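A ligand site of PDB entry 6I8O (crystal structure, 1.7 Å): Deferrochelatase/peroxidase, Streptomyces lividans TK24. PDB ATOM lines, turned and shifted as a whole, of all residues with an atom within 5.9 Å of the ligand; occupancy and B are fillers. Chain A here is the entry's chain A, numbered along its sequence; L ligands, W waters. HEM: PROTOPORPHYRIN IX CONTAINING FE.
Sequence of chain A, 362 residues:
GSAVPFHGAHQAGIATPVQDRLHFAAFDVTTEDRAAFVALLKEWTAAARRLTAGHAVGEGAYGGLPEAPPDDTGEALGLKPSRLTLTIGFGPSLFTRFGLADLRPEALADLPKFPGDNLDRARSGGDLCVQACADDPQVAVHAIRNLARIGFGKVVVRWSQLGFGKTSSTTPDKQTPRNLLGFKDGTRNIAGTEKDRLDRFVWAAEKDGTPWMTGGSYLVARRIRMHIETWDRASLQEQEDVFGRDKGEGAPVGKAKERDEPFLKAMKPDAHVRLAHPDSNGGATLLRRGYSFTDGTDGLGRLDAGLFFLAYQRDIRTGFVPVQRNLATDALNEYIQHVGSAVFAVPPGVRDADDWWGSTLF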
ATOM      1  N   ASN A 179      19.395 -12.261  32.592  1.00  0.00           N
ATOM      2  CA  ASN A 179      18.746 -13.068  33.609  1.00  0.00           C
ATOM      3  C   ASN A 179      19.316 -12.686  34.988  1.00  0.00           C
ATOM      4  O   ASN A 179      20.158 -11.783  35.105  1.00  0.00           O
ATOM      5  CB  ASN A 179      18.927 -14.554  33.298  1.00  0.00           C
ATOM      6  CG  ASN A 179      20.393 -14.932  33.113  1.00  0.00           C
ATOM      7  OD1 ASN A 179      21.228 -14.569  33.932  1.00  0.00           O
ATOM      8  ND2 ASN A 179      20.695 -15.643  32.038  1.00  0.00           N
ATOM      9  N   LEU A 181      21.363 -14.188  36.922  1.00  0.00           N
ATOM     10  CA  LEU A 181      22.799 -14.351  37.110  1.00  0.00           C
ATOM     11  C   LEU A 181      23.609 -13.228  36.501  1.00  0.00           C
ATOM     12  O   LEU A 181      24.836 -13.214  36.639  1.00  0.00           O
ATOM     13  CB  LEU A 181      23.267 -15.687  36.524  1.00  0.00           C
ATOM     14  CG  LEU A 181      22.452 -16.861  37.033  1.00  0.00           C
ATOM     15  CD1 LEU A 181      22.955 -18.161  36.416  1.00  0.00           C
ATOM     16  CD2 LEU A 181      22.549 -16.908  38.535  1.00  0.00           C
ATOM     17  N   PHE A 183      23.850 -12.363  33.193  1.00  0.00           N
ATOM     18  CA  PHE A 183      24.295 -12.542  31.825  1.00  0.00           C
ATOM     19  C   PHE A 183      23.163 -12.277  30.835  1.00  0.00           C
ATOM     20  O   PHE A 183      21.996 -12.579  31.105  1.00  0.00           O
ATOM     21  CB  PHE A 183      24.865 -13.939  31.605  1.00  0.00           C
ATOM     22  CG  PHE A 183      26.274 -14.121  32.110  1.00  0.00           C
ATOM     23  CD1 PHE A 183      26.527 -14.206  33.469  1.00  0.00           C
ATOM     24  CD2 PHE A 183      27.329 -14.231  31.220  1.00  0.00           C
ATOM     25  CE1 PHE A 183      27.832 -14.377  33.943  1.00  0.00           C
ATOM     26  CE2 PHE A 183      28.632 -14.414  31.685  1.00  0.00           C
ATOM     27  CZ  PHE A 183      28.883 -14.469  33.040  1.00  0.00           C
ATOM     28  N   LYS A 184      23.518 -11.699  29.688  1.00  0.00           N
ATOM     29  CA  LYS A 184      22.578 -11.618  28.580  1.00  0.00           C
ATOM     30  C   LYS A 184      22.087 -13.012  28.232  1.00  0.00           C
ATOM     31  O   LYS A 184      22.861 -13.981  28.247  1.00  0.00           O
ATOM     32  CB  LYS A 184      23.229 -10.982  27.353  1.00  0.00           C
ATOM     33  CG  LYS A 184      23.597  -9.538  27.522  1.00  0.00           C
ATOM     34  CD  LYS A 184      24.366  -9.031  26.293  1.00  0.00           C
ATOM     35  CE  LYS A 184      24.656  -7.535  26.452  1.00  0.00           C
ATOM     36  NZ  LYS A 184      25.492  -7.033  25.340  1.00  0.00           N
ATOM     37  N   ASP A 185      20.802 -13.119  27.907  1.00  0.00           N
ATOM     38  CA  ASP A 185      20.152 -14.405  27.653  1.00  0.00           C
ATOM     39  C   ASP A 185      19.271 -14.231  26.434  1.00  0.00           C
ATOM     40  O   ASP A 185      18.247 -13.536  26.510  1.00  0.00           O
ATOM     41  CB  ASP A 185      19.329 -14.840  28.877  1.00  0.00           C
ATOM     42  CG  ASP A 185      19.163 -16.353  29.020  1.00  0.00           C
ATOM     43  OD1 ASP A 185      19.219 -17.117  28.022  1.00  0.00           O
ATOM     44  OD2 ASP A 185      18.938 -16.775  30.185  1.00  0.00           O
ATOM     45  N   GLY A 186      19.634 -14.874  25.316  1.00  0.00           N
ATOM     46  CA  GLY A 186      18.809 -14.808  24.114  1.00  0.00           C
ATOM     47  C   GLY A 186      19.553 -14.430  22.838  1.00  0.00           C
ATOM     48  O   GLY A 186      18.954 -14.305  21.770  1.00  0.00           O
ATOM     49  N   THR A 187      20.879 -14.284  22.936  1.00  0.00           N
ATOM     50  CA  THR A 187      21.665 -13.786  21.802  1.00  0.00           C
ATOM     51  C   THR A 187      21.521 -14.699  20.583  1.00  0.00           C
ATOM     52  O   THR A 187      21.126 -14.253  19.500  1.00  0.00           O
ATOM     53  CB  THR A 187      23.124 -13.647  22.222  1.00  0.00           C
ATOM     54  OG1 THR A 187      23.185 -12.826  23.388  1.00  0.00           O
ATOM     55  CG2 THR A 187      23.954 -13.033  21.115  1.00  0.00           C
ATOM     56  N   ARG A 188      21.838 -15.983  20.732  1.00  0.00           N
ATOM     57  CA  ARG A 188      21.737 -16.921  19.625  1.00  0.00           C
ATOM     58  C   ARG A 188      20.467 -17.745  19.829  1.00  0.00           C
ATOM     59  O   ARG A 188      20.475 -18.873  20.309  1.00  0.00           O
ATOM     60  CB  ARG A 188      23.010 -17.774  19.531  1.00  0.00           C
ATOM     61  CG  ARG A 188      24.186 -16.996  18.898  1.00  0.00           C
ATOM     62  CD  ARG A 188      25.402 -17.896  18.590  1.00  0.00           C
ATOM     63  NE  ARG A 188      24.983 -19.286  18.452  1.00  0.00           N
ATOM     64  CZ  ARG A 188      24.557 -19.809  17.314  1.00  0.00           C
ATOM     65  NH1 ARG A 188      24.155 -21.069  17.261  1.00  0.00           N
ATOM     66  NH2 ARG A 188      24.547 -19.074  16.206  1.00  0.00           N
ATOM     67  N   ASN A 189      19.331 -17.127  19.476  1.00  0.00           N
ATOM     68  CA  ASN A 189      18.024 -17.766  19.460  1.00  0.00           C
ATOM     69  C   ASN A 189      17.552 -17.829  18.002  1.00  0.00           C
ATOM     70  O   ASN A 189      18.364 -17.699  17.078  1.00  0.00           O
ATOM     71  CB  ASN A 189      17.073 -16.977  20.381  1.00  0.00           C
ATOM     72  CG  ASN A 189      15.947 -17.826  20.933  1.00  0.00           C
ATOM     73  OD1 ASN A 189      16.103 -19.024  21.134  1.00  0.00           O
ATOM     74  ND2 ASN A 189      14.801 -17.203  21.163  1.00  0.00           N
ATOM     75  N   ILE A 224      13.143 -23.546  37.040  1.00  0.00           N
ATOM     76  CA  ILE A 224      14.527 -23.769  37.474  1.00  0.00           C
ATOM     77  C   ILE A 224      14.867 -22.813  38.602  1.00  0.00           C
ATOM     78  O   ILE A 224      14.863 -21.596  38.409  1.00  0.00           O
ATOM     79  CB  ILE A 224      15.525 -23.587  36.328  1.00  0.00           C
ATOM     80  CG1 ILE A 224      15.120 -24.469  35.146  1.00  0.00           C
ATOM     81  CG2 ILE A 224      16.924 -23.948  36.815  1.00  0.00           C
ATOM     82  CD1 ILE A 224      15.978 -24.184  33.906  1.00  0.00           C
ATOM     83  N   MET A 226      17.587 -21.030  41.039  1.00  0.00           N
ATOM     84  CA  MET A 226      18.981 -20.594  40.982  1.00  0.00           C
ATOM     85  C   MET A 226      19.539 -20.491  42.406  1.00  0.00           C
ATOM     86  O   MET A 226      18.885 -19.925  43.293  1.00  0.00           O
ATOM     87  CB  MET A 226      19.105 -19.248  40.268  1.00  0.00           C
ATOM     88  CG  MET A 226      18.731 -19.330  38.797  1.00  0.00           C
ATOM     89  SD  MET A 226      18.508 -17.650  38.153  1.00  0.00           S
ATOM     90  CE  MET A 226      18.984 -17.886  36.450  1.00  0.00           C
ATOM     91  N   PHE A 243      29.784 -20.048  31.414  1.00  0.00           N
ATOM     92  CA  PHE A 243      28.985 -19.851  30.209  1.00  0.00           C
ATOM     93  C   PHE A 243      29.787 -19.919  28.919  1.00  0.00           C
ATOM     94  O   PHE A 243      29.295 -20.470  27.926  1.00  0.00           O
ATOM     95  CB  PHE A 243      28.261 -18.512  30.305  1.00  0.00           C
ATOM     96  CG  PHE A 243      27.090 -18.554  31.219  1.00  0.00           C
ATOM     97  CD1 PHE A 243      25.967 -19.321  30.902  1.00  0.00           C
ATOM     98  CD2 PHE A 243      27.104 -17.856  32.415  1.00  0.00           C
ATOM     99  CE1 PHE A 243      24.879 -19.393  31.769  1.00  0.00           C
ATOM    100  CE2 PHE A 243      26.018 -17.916  33.290  1.00  0.00           C
ATOM    101  CZ  PHE A 243      24.903 -18.678  32.953  1.00  0.00           C
ATOM    102  N   ARG A 245      30.939 -16.917  27.650  1.00  0.00           N
ATOM    103  CA  ARG A 245      30.867 -15.535  27.220  1.00  0.00           C
ATOM    104  C   ARG A 245      31.226 -14.630  28.388  1.00  0.00           C
ATOM    105  O   ARG A 245      31.085 -15.005  29.560  1.00  0.00           O
ATOM    106  CB  ARG A 245      29.468 -15.180  26.717  1.00  0.00           C
ATOM    107  CG  ARG A 245      29.002 -15.947  25.473  1.00  0.00           C
ATOM    108  CD  ARG A 245      27.583 -15.557  25.129  1.00  0.00           C
ATOM    109  NE  ARG A 245      27.053 -16.168  23.901  1.00  0.00           N
ATOM    110  CZ  ARG A 245      27.122 -15.601  22.695  1.00  0.00           C
ATOM    111  NH1 ARG A 245      27.718 -14.431  22.550  1.00  0.00           N
ATOM    112  NH2 ARG A 245      26.596 -16.204  21.635  1.00  0.00           N
ATOM    113  N   PRO A 262      30.461 -17.640  18.204  1.00  0.00           N
ATOM    114  CA  PRO A 262      31.333 -18.328  19.165  1.00  0.00           C
ATOM    115  C   PRO A 262      32.324 -19.236  18.461  1.00  0.00           C
ATOM    116  O   PRO A 262      32.042 -19.828  17.417  1.00  0.00           O
ATOM    117  CB  PRO A 262      30.359 -19.145  20.032  1.00  0.00           C
ATOM    118  CG  PRO A 262      29.030 -19.089  19.336  1.00  0.00           C
ATOM    119  CD  PRO A 262      29.030 -17.898  18.433  1.00  0.00           C
ATOM    120  N   HIS A 272      28.532 -23.822  29.294  1.00  0.00           N
ATOM    121  CA  HIS A 272      27.128 -23.964  28.941  1.00  0.00           C
ATOM    122  C   HIS A 272      26.899 -23.793  27.449  1.00  0.00           C
ATOM    123  O   HIS A 272      26.222 -24.608  26.810  1.00  0.00           O
ATOM    124  CB  HIS A 272      26.306 -22.958  29.725  1.00  0.00           C
ATOM    125  CG  HIS A 272      24.843 -23.047  29.465  1.00  0.00           C
ATOM    126  ND1 HIS A 272      24.071 -24.086  29.916  1.00  0.00           N
ATOM    127  CD2 HIS A 272      24.005 -22.211  28.813  1.00  0.00           C
ATOM    128  CE1 HIS A 272      22.816 -23.899  29.546  1.00  0.00           C
ATOM    129  NE2 HIS A 272      22.751 -22.760  28.881  1.00  0.00           N
ATOM    130  N   VAL A 273      27.463 -22.734  26.860  1.00  0.00           N
ATOM    131  CA  VAL A 273      27.258 -22.433  25.439  1.00  0.00           C
ATOM    132  C   VAL A 273      27.864 -23.517  24.570  1.00  0.00           C
ATOM    133  O   VAL A 273      27.280 -23.914  23.551  1.00  0.00           O
ATOM    134  CB  VAL A 273      27.839 -21.054  25.096  1.00  0.00           C
ATOM    135  CG1 VAL A 273      27.850 -20.853  23.607  1.00  0.00           C
ATOM    136  CG2 VAL A 273      27.044 -19.975  25.799  1.00  0.00           C
ATOM    137  N   ALA A 276      25.451 -26.479  24.721  1.00  0.00           N
ATOM    138  CA  ALA A 276      24.117 -26.227  24.190  1.00  0.00           C
ATOM    139  C   ALA A 276      24.088 -25.904  22.709  1.00  0.00           C
ATOM    140  O   ALA A 276      23.024 -25.975  22.094  1.00  0.00           O
ATOM    141  CB  ALA A 276      23.454 -25.063  24.960  1.00  0.00           C
ATOM    142  N   HIS A 277      25.223 -25.540  22.133  1.00  0.00           N
ATOM    143  CA  HIS A 277      25.260 -25.030  20.771  1.00  0.00           C
ATOM    144  C   HIS A 277      24.724 -26.082  19.795  1.00  0.00           C
ATOM    145  O   HIS A 277      24.951 -27.279  20.008  1.00  0.00           O
ATOM    146  CB  HIS A 277      26.700 -24.643  20.412  1.00  0.00           C
ATOM    147  CG  HIS A 277      26.827 -23.775  19.195  1.00  0.00           C
ATOM    148  ND1 HIS A 277      26.880 -24.272  17.918  1.00  0.00           N
ATOM    149  CD2 HIS A 277      26.960 -22.433  19.086  1.00  0.00           C
ATOM    150  CE1 HIS A 277      27.008 -23.274  17.066  1.00  0.00           C
ATOM    151  NE2 HIS A 277      27.057 -22.148  17.744  1.00  0.00           N
ATOM    152  N   PRO A 278      23.976 -25.685  18.766  1.00  0.00           N
ATOM    153  CA  PRO A 278      23.528 -26.674  17.774  1.00  0.00           C
ATOM    154  C   PRO A 278      24.649 -27.581  17.274  1.00  0.00           C
ATOM    155  O   PRO A 278      24.430 -28.784  17.113  1.00  0.00           O
ATOM    156  CB  PRO A 278      22.961 -25.794  16.645  1.00  0.00           C
ATOM    157  CG  PRO A 278      22.475 -24.561  17.328  1.00  0.00           C
ATOM    158  CD  PRO A 278      23.282 -24.393  18.609  1.00  0.00           C
ATOM    159  N   LEU A 286      16.636 -24.634  19.275  1.00  0.00           N
ATOM    160  CA  LEU A 286      15.459 -24.342  20.094  1.00  0.00           C
ATOM    161  C   LEU A 286      15.038 -22.896  19.910  1.00  0.00           C
ATOM    162  O   LEU A 286      15.865 -22.036  19.598  1.00  0.00           O
ATOM    163  CB  LEU A 286      15.735 -24.590  21.587  1.00  0.00           C
ATOM    164  CG  LEU A 286      16.200 -25.992  21.944  1.00  0.00           C
ATOM    165  CD1 LEU A 286      16.443 -26.072  23.429  1.00  0.00           C
ATOM    166  CD2 LEU A 286      15.112 -26.943  21.487  1.00  0.00           C
ATOM    167  N   ARG A 288      13.943 -20.347  22.408  1.00  0.00           N
ATOM    168  CA  ARG A 288      13.846 -20.068  23.833  1.00  0.00           C
ATOM    169  C   ARG A 288      12.983 -18.821  24.067  1.00  0.00           C
ATOM    170  O   ARG A 288      13.129 -17.816  23.358  1.00  0.00           O
ATOM    171  CB  ARG A 288      15.242 -19.881  24.427  1.00  0.00           C
ATOM    172  CG  ARG A 288      15.983 -21.197  24.573  1.00  0.00           C
ATOM    173  CD  ARG A 288      17.433 -20.980  24.949  1.00  0.00           C
ATOM    174  NE  ARG A 288      18.160 -20.277  23.905  1.00  0.00           N
ATOM    175  CZ  ARG A 288      19.012 -19.282  24.113  1.00  0.00           C
ATOM    176  NH1 ARG A 288      19.273 -18.848  25.339  1.00  0.00           N
ATOM    177  NH2 ARG A 288      19.640 -18.722  23.077  1.00  0.00           N
ATOM    178  N   LEU A 307      14.422 -19.098  37.071  1.00  0.00           N
ATOM    179  CA  LEU A 307      14.184 -18.874  35.652  1.00  0.00           C
ATOM    180  C   LEU A 307      13.106 -19.845  35.220  1.00  0.00           C
ATOM    181  O   LEU A 307      13.252 -21.070  35.401  1.00  0.00           O
ATOM    182  CB  LEU A 307      15.469 -19.054  34.842  1.00  0.00           C
ATOM    183  CG  LEU A 307      15.374 -18.640  33.381  1.00  0.00           C
ATOM    184  CD1 LEU A 307      16.623 -17.904  32.963  1.00  0.00           C
ATOM    185  CD2 LEU A 307      15.155 -19.850  32.496  1.00  0.00           C
ATOM    186  N   PHE A 309      11.798 -21.493  32.352  1.00  0.00           N
ATOM    187  CA  PHE A 309      12.358 -21.759  31.035  1.00  0.00           C
ATOM    188  C   PHE A 309      11.293 -22.345  30.125  1.00  0.00           C
ATOM    189  O   PHE A 309      10.626 -23.327  30.470  1.00  0.00           O
ATOM    190  CB  PHE A 309      13.550 -22.727  31.183  1.00  0.00           C
ATOM    191  CG  PHE A 309      14.214 -23.101  29.889  1.00  0.00           C
ATOM    192  CD1 PHE A 309      15.272 -22.366  29.396  1.00  0.00           C
ATOM    193  CD2 PHE A 309      13.807 -24.235  29.208  1.00  0.00           C
ATOM    194  CE1 PHE A 309      15.902 -22.719  28.187  1.00  0.00           C
ATOM    195  CE2 PHE A 309      14.418 -24.615  28.015  1.00  0.00           C
ATOM    196  CZ  PHE A 309      15.470 -23.872  27.500  1.00  0.00           C
ATOM    197  N   PHE A 320      14.444 -30.306  22.723  1.00  0.00           N
ATOM    198  CA  PHE A 320      14.830 -30.155  24.122  1.00  0.00           C
ATOM    199  C   PHE A 320      15.614 -31.354  24.618  1.00  0.00           C
ATOM    200  O   PHE A 320      16.607 -31.204  25.341  1.00  0.00           O
ATOM    201  CB  PHE A 320      13.594 -29.919  24.991  1.00  0.00           C
ATOM    202  CG  PHE A 320      13.912 -29.834  26.444  1.00  0.00           C
ATOM    203  CD1 PHE A 320      14.388 -28.644  26.990  1.00  0.00           C
ATOM    204  CD2 PHE A 320      13.762 -30.938  27.266  1.00  0.00           C
ATOM    205  CE1 PHE A 320      14.709 -28.559  28.345  1.00  0.00           C
ATOM    206  CE2 PHE A 320      14.074 -30.868  28.608  1.00  0.00           C
ATOM    207  CZ  PHE A 320      14.552 -29.673  29.146  1.00  0.00           C
ATOM    208  N   VAL A 323      19.468 -31.719  23.537  1.00  0.00           N
ATOM    209  CA  VAL A 323      20.222 -30.629  24.136  1.00  0.00           C
ATOM    210  C   VAL A 323      20.286 -30.806  25.652  1.00  0.00           C
ATOM    211  O   VAL A 323      21.368 -30.708  26.251  1.00  0.00           O
ATOM    212  CB  VAL A 323      19.609 -29.263  23.758  1.00  0.00           C
ATOM    213  CG1 VAL A 323      20.456 -28.122  24.368  1.00  0.00           C
ATOM    214  CG2 VAL A 323      19.543 -29.109  22.225  1.00  0.00           C
ATOM    215  N   GLN A 324      19.153 -31.089  26.299  1.00  0.00           N
ATOM    216  CA  GLN A 324      19.220 -31.202  27.762  1.00  0.00           C
ATOM    217  C   GLN A 324      20.039 -32.417  28.189  1.00  0.00           C
ATOM    218  O   GLN A 324      20.708 -32.365  29.220  1.00  0.00           O
ATOM    219  CB  GLN A 324      17.809 -31.240  28.362  1.00  0.00           C
ATOM    220  CG  GLN A 324      17.762 -31.541  29.885  1.00  0.00           C
ATOM    221  CD  GLN A 324      18.346 -30.425  30.777  1.00  0.00           C
ATOM    222  OE1 GLN A 324      18.354 -29.260  30.412  1.00  0.00           O
ATOM    223  NE2 GLN A 324      18.812 -30.806  31.964  1.00  0.00           N
ATOM    224  N   LEU A 327      23.540 -31.520  28.511  1.00  0.00           N
ATOM    225  CA  LEU A 327      23.855 -30.637  29.621  1.00  0.00           C
ATOM    226  C   LEU A 327      24.170 -31.395  30.902  1.00  0.00           C
ATOM    227  O   LEU A 327      24.351 -30.765  31.947  1.00  0.00           O
ATOM    228  CB  LEU A 327      22.696 -29.656  29.858  1.00  0.00           C
ATOM    229  CG  LEU A 327      22.448 -28.642  28.733  1.00  0.00           C
ATOM    230  CD1 LEU A 327      21.488 -27.524  29.182  1.00  0.00           C
ATOM    231  CD2 LEU A 327      23.757 -28.053  28.229  1.00  0.00           C
ATOM    232  N   LEU A 332      27.077 -25.193  34.589  1.00  0.00           N
ATOM    233  CA  LEU A 332      25.966 -24.446  35.173  1.00  0.00           C
ATOM    234  C   LEU A 332      25.199 -25.278  36.194  1.00  0.00           C
ATOM    235  O   LEU A 332      24.560 -24.714  37.082  1.00  0.00           O
ATOM    236  CB  LEU A 332      25.024 -23.979  34.069  1.00  0.00           C
ATOM    237  CG  LEU A 332      23.842 -23.121  34.477  1.00  0.00           C
ATOM    238  CD1 LEU A 332      24.339 -21.896  35.199  1.00  0.00           C
ATOM    239  CD2 LEU A 332      22.999 -22.731  33.256  1.00  0.00           C
ATOM    240  N   ILE A 336      22.048 -24.394  39.623  1.00  0.00           N
ATOM    241  CA  ILE A 336      20.635 -24.448  39.282  1.00  0.00           C
ATOM    242  C   ILE A 336      20.083 -25.804  39.709  1.00  0.00           C
ATOM    243  O   ILE A 336      20.817 -26.742  39.989  1.00  0.00           O
ATOM    244  CB  ILE A 336      20.385 -24.227  37.773  1.00  0.00           C
ATOM    245  CG1 ILE A 336      21.067 -25.323  36.943  1.00  0.00           C
ATOM    246  CG2 ILE A 336      20.860 -22.860  37.357  1.00  0.00           C
ATOM    247  CD1 ILE A 336      20.506 -25.455  35.510  1.00  0.00           C
ATOM    248  N   HIS A 338      16.362 -28.056  38.521  1.00  0.00           N
ATOM    249  CA  HIS A 338      15.053 -28.109  37.862  1.00  0.00           C
ATOM    250  C   HIS A 338      14.036 -28.653  38.857  1.00  0.00           C
ATOM    251  O   HIS A 338      14.178 -29.789  39.337  1.00  0.00           O
ATOM    252  CB  HIS A 338      15.090 -29.007  36.629  1.00  0.00           C
ATOM    253  CG  HIS A 338      15.957 -28.480  35.526  1.00  0.00           C
ATOM    254  ND1 HIS A 338      15.490 -28.277  34.235  1.00  0.00           N
ATOM    255  CD2 HIS A 338      17.256 -28.101  35.515  1.00  0.00           C
ATOM    256  CE1 HIS A 338      16.467 -27.813  33.486  1.00  0.00           C
ATOM    257  NE2 HIS A 338      17.559 -27.718  34.233  1.00  0.00           N
HETATM  258  CHA HEM L   1      22.589 -19.878  25.640  1.00  0.00           C
HETATM  259  CHB HEM L   1      21.942 -19.037  30.378  1.00  0.00           C
HETATM  260  CHC HEM L   1      19.220 -22.991  30.804  1.00  0.00           C
HETATM  261  CHD HEM L   1      19.874 -23.874  26.074  1.00  0.00           C
HETATM  262  C1A HEM L   1      22.640 -19.309  26.885  1.00  0.00           C
HETATM  263  C2A HEM L   1      23.385 -18.132  27.248  1.00  0.00           C
HETATM  264  C3A HEM L   1      23.209 -17.933  28.555  1.00  0.00           C
HETATM  265  C4A HEM L   1      22.352 -18.954  29.069  1.00  0.00           C
HETATM  266  CMA HEM L   1      23.790 -16.798  29.410  1.00  0.00           C
HETATM  267  CAA HEM L   1      24.243 -17.297  26.291  1.00  0.00           C
HETATM  268  CBA HEM L   1      23.506 -16.308  25.390  1.00  0.00           C
HETATM  269  CGA HEM L   1      22.486 -16.889  24.441  1.00  0.00           C
HETATM  270  O1A HEM L   1      21.308 -16.987  24.855  1.00  0.00           O
HETATM  271  O2A HEM L   1      22.843 -17.192  23.269  1.00  0.00           O
HETATM  272  C1B HEM L   1      21.103 -19.985  30.898  1.00  0.00           C
HETATM  273  C2B HEM L   1      20.590 -20.030  32.257  1.00  0.00           C
HETATM  274  C3B HEM L   1      19.846 -21.143  32.374  1.00  0.00           C
HETATM  275  C4B HEM L   1      19.874 -21.823  31.085  1.00  0.00           C
HETATM  276  CMB HEM L   1      20.877 -18.955  33.327  1.00  0.00           C
HETATM  277  CAB HEM L   1      19.038 -21.686  33.572  1.00  0.00           C
HETATM  278  CBB HEM L   1      18.843 -20.968  34.679  1.00  0.00           C
HETATM  279  C1C HEM L   1      19.171 -23.596  29.571  1.00  0.00           C
HETATM  280  C2C HEM L   1      18.526 -24.858  29.260  1.00  0.00           C
HETATM  281  C3C HEM L   1      18.711 -25.098  27.936  1.00  0.00           C
HETATM  282  C4C HEM L   1      19.479 -24.005  27.387  1.00  0.00           C
HETATM  283  CMC HEM L   1      17.767 -25.679  30.326  1.00  0.00           C
HETATM  284  CAC HEM L   1      18.242 -26.296  27.088  1.00  0.00           C
HETATM  285  CBC HEM L   1      17.751 -27.395  27.658  1.00  0.00           C
HETATM  286  C1D HEM L   1      20.618 -22.854  25.532  1.00  0.00           C
HETATM  287  C2D HEM L   1      20.938 -22.670  24.134  1.00  0.00           C
HETATM  288  C3D HEM L   1      21.694 -21.569  24.010  1.00  0.00           C
HETATM  289  C4D HEM L   1      21.884 -21.015  25.325  1.00  0.00           C
HETATM  290  CMD HEM L   1      20.500 -23.570  22.960  1.00  0.00           C
HETATM  291  CAD HEM L   1      22.259 -21.013  22.678  1.00  0.00           C
HETATM  292  CBD HEM L   1      23.657 -21.573  22.440  1.00  0.00           C
HETATM  293  CGD HEM L   1      24.136 -21.179  21.066  1.00  0.00           C
HETATM  294  O1D HEM L   1      25.112 -20.379  20.966  1.00  0.00           O
HETATM  295  O2D HEM L   1      23.516 -21.665  20.089  1.00  0.00           O
HETATM  296  NA  HEM L   1      22.018 -19.807  28.029  1.00  0.00           N
HETATM  297  NB  HEM L   1      20.655 -21.095  30.239  1.00  0.00           N
HETATM  298  NC  HEM L   1      19.733 -23.118  28.417  1.00  0.00           N
HETATM  299  ND  HEM L   1      21.205 -21.811  26.222  1.00  0.00           N
HETATM  300 FE   HEM L   1      20.965 -21.502  28.256  1.00  0.00          FE
HETATM  301  O   HOH W   1      25.209 -18.279  22.808  1.00  0.00           O
HETATM  302  O   HOH W   2      18.937 -20.057  28.017  1.00  0.00           O
HETATM  303  O   HOH W   3      21.086 -21.512  19.192  1.00  0.00           O
HETATM  304  O   HOH W   4      20.480 -25.901  20.567  1.00  0.00           O
HETATM  305  O   HOH W   5      19.228 -23.606  20.002  1.00  0.00           O
HETATM  306  O   HOH W   6      17.843 -19.333  30.035  1.00  0.00           O
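The side-chain amide nitrogen (ND2) of Asn 179 is in hydrogen-bond range of the backbone carbonyl oxygen (O) of Phe 183, at 3.5 Å. The side-chain amide oxygen of Asn 179 sits at hydrogen-bond distance from the backbone NH of Leu 181, at 3.0 Å. NE2 of His 277 is in hydrogen-bond range of NH1 of Arg 188. The backbone NH of Leu 307 sits at hydrogen-bond distance from the backbone carbonyl oxygen of Ile 224, 2.9 Å away. The side-chain amide nitrogen (ND2) of Asn 179 lies within hydrogen-bond range of the side-chain carboxylate (OD2) of Asp 185, 2.8 Å away. O of Arg 288 is in hydrogen-bond range of ND2 of Asn 189, 2.8 Å away. The guanidinium group (NH1) of Arg 288 lies within salt-bridge range of the side-chain carboxylate (OD1) of Asp 185, 3.2 Å away. NH2 of Arg 288 lies within hydrogen-bond range of O of Arg 188, 2.9 Å away.
Water W2 lies within hydrogen-bond range of the side-chain carboxylate of Asp 185 (3.0 Å) and the guanidinium group of Arg 288 (3.0 Å). Water W3 lies within hydrogen-bond range of an oxygen (O2D) of the ligand (2.6 Å) and the backbone carbonyl oxygen of Arg 188 (2.9 Å). Water W1 lies within hydrogen-bond range of an oxygen (O2A) of the ligand and the guanidinium group of Arg 245.
NE of Arg 188 lies within salt-bridge range of O1D of the ligand (2.7 Å). NE2 of His 272 is bound to FE of the ligand, at 2.3 Å. N of Gly 186 lies within hydrogen-bond range of O1A of the ligand, 2.7 Å away. O1A of the ligand is in salt-bridge range of NH1 of Arg 288 (2.8 Å). N of Thr 187 sits at hydrogen-bond distance from O1A of the ligand (3.3 Å). An oxygen (O2A) of the ligand sits at hydrogen-bond distance from the backbone NH (N) of Arg 188, 3.0 Å away.
Residues that only touch the ligand: Pro 278 (3.1 Å), Lys 184 (3.2 Å), Phe 243 (3.3 Å), Phe 320 (3.3 Å), His 277 (3.3 Å), Gln 324 (3.4 Å), Phe 309 (3.5 Å), Met 226 (3.6 Å), Asn 179 (3.6 Å), Ala 276 (3.6 Å), Leu 332 (3.6 Å), Phe 183 (3.8 Å), Asp 185 (3.8 Å), Leu 181 (3.8 Å), Val 273 (3.8 Å), Arg 245 (3.8 Å), Ile 336 (3.8 Å), Leu 307 (3.9 Å), Leu 327 (3.9 Å), Val 323 (3.95 Å) and Ile 224 (3.96 Å). Of the 30 residues printed, 26 come within 4 Å of the ligand. The nearest printed residue that does not touch the ligand is His 338 (4.03 Å).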
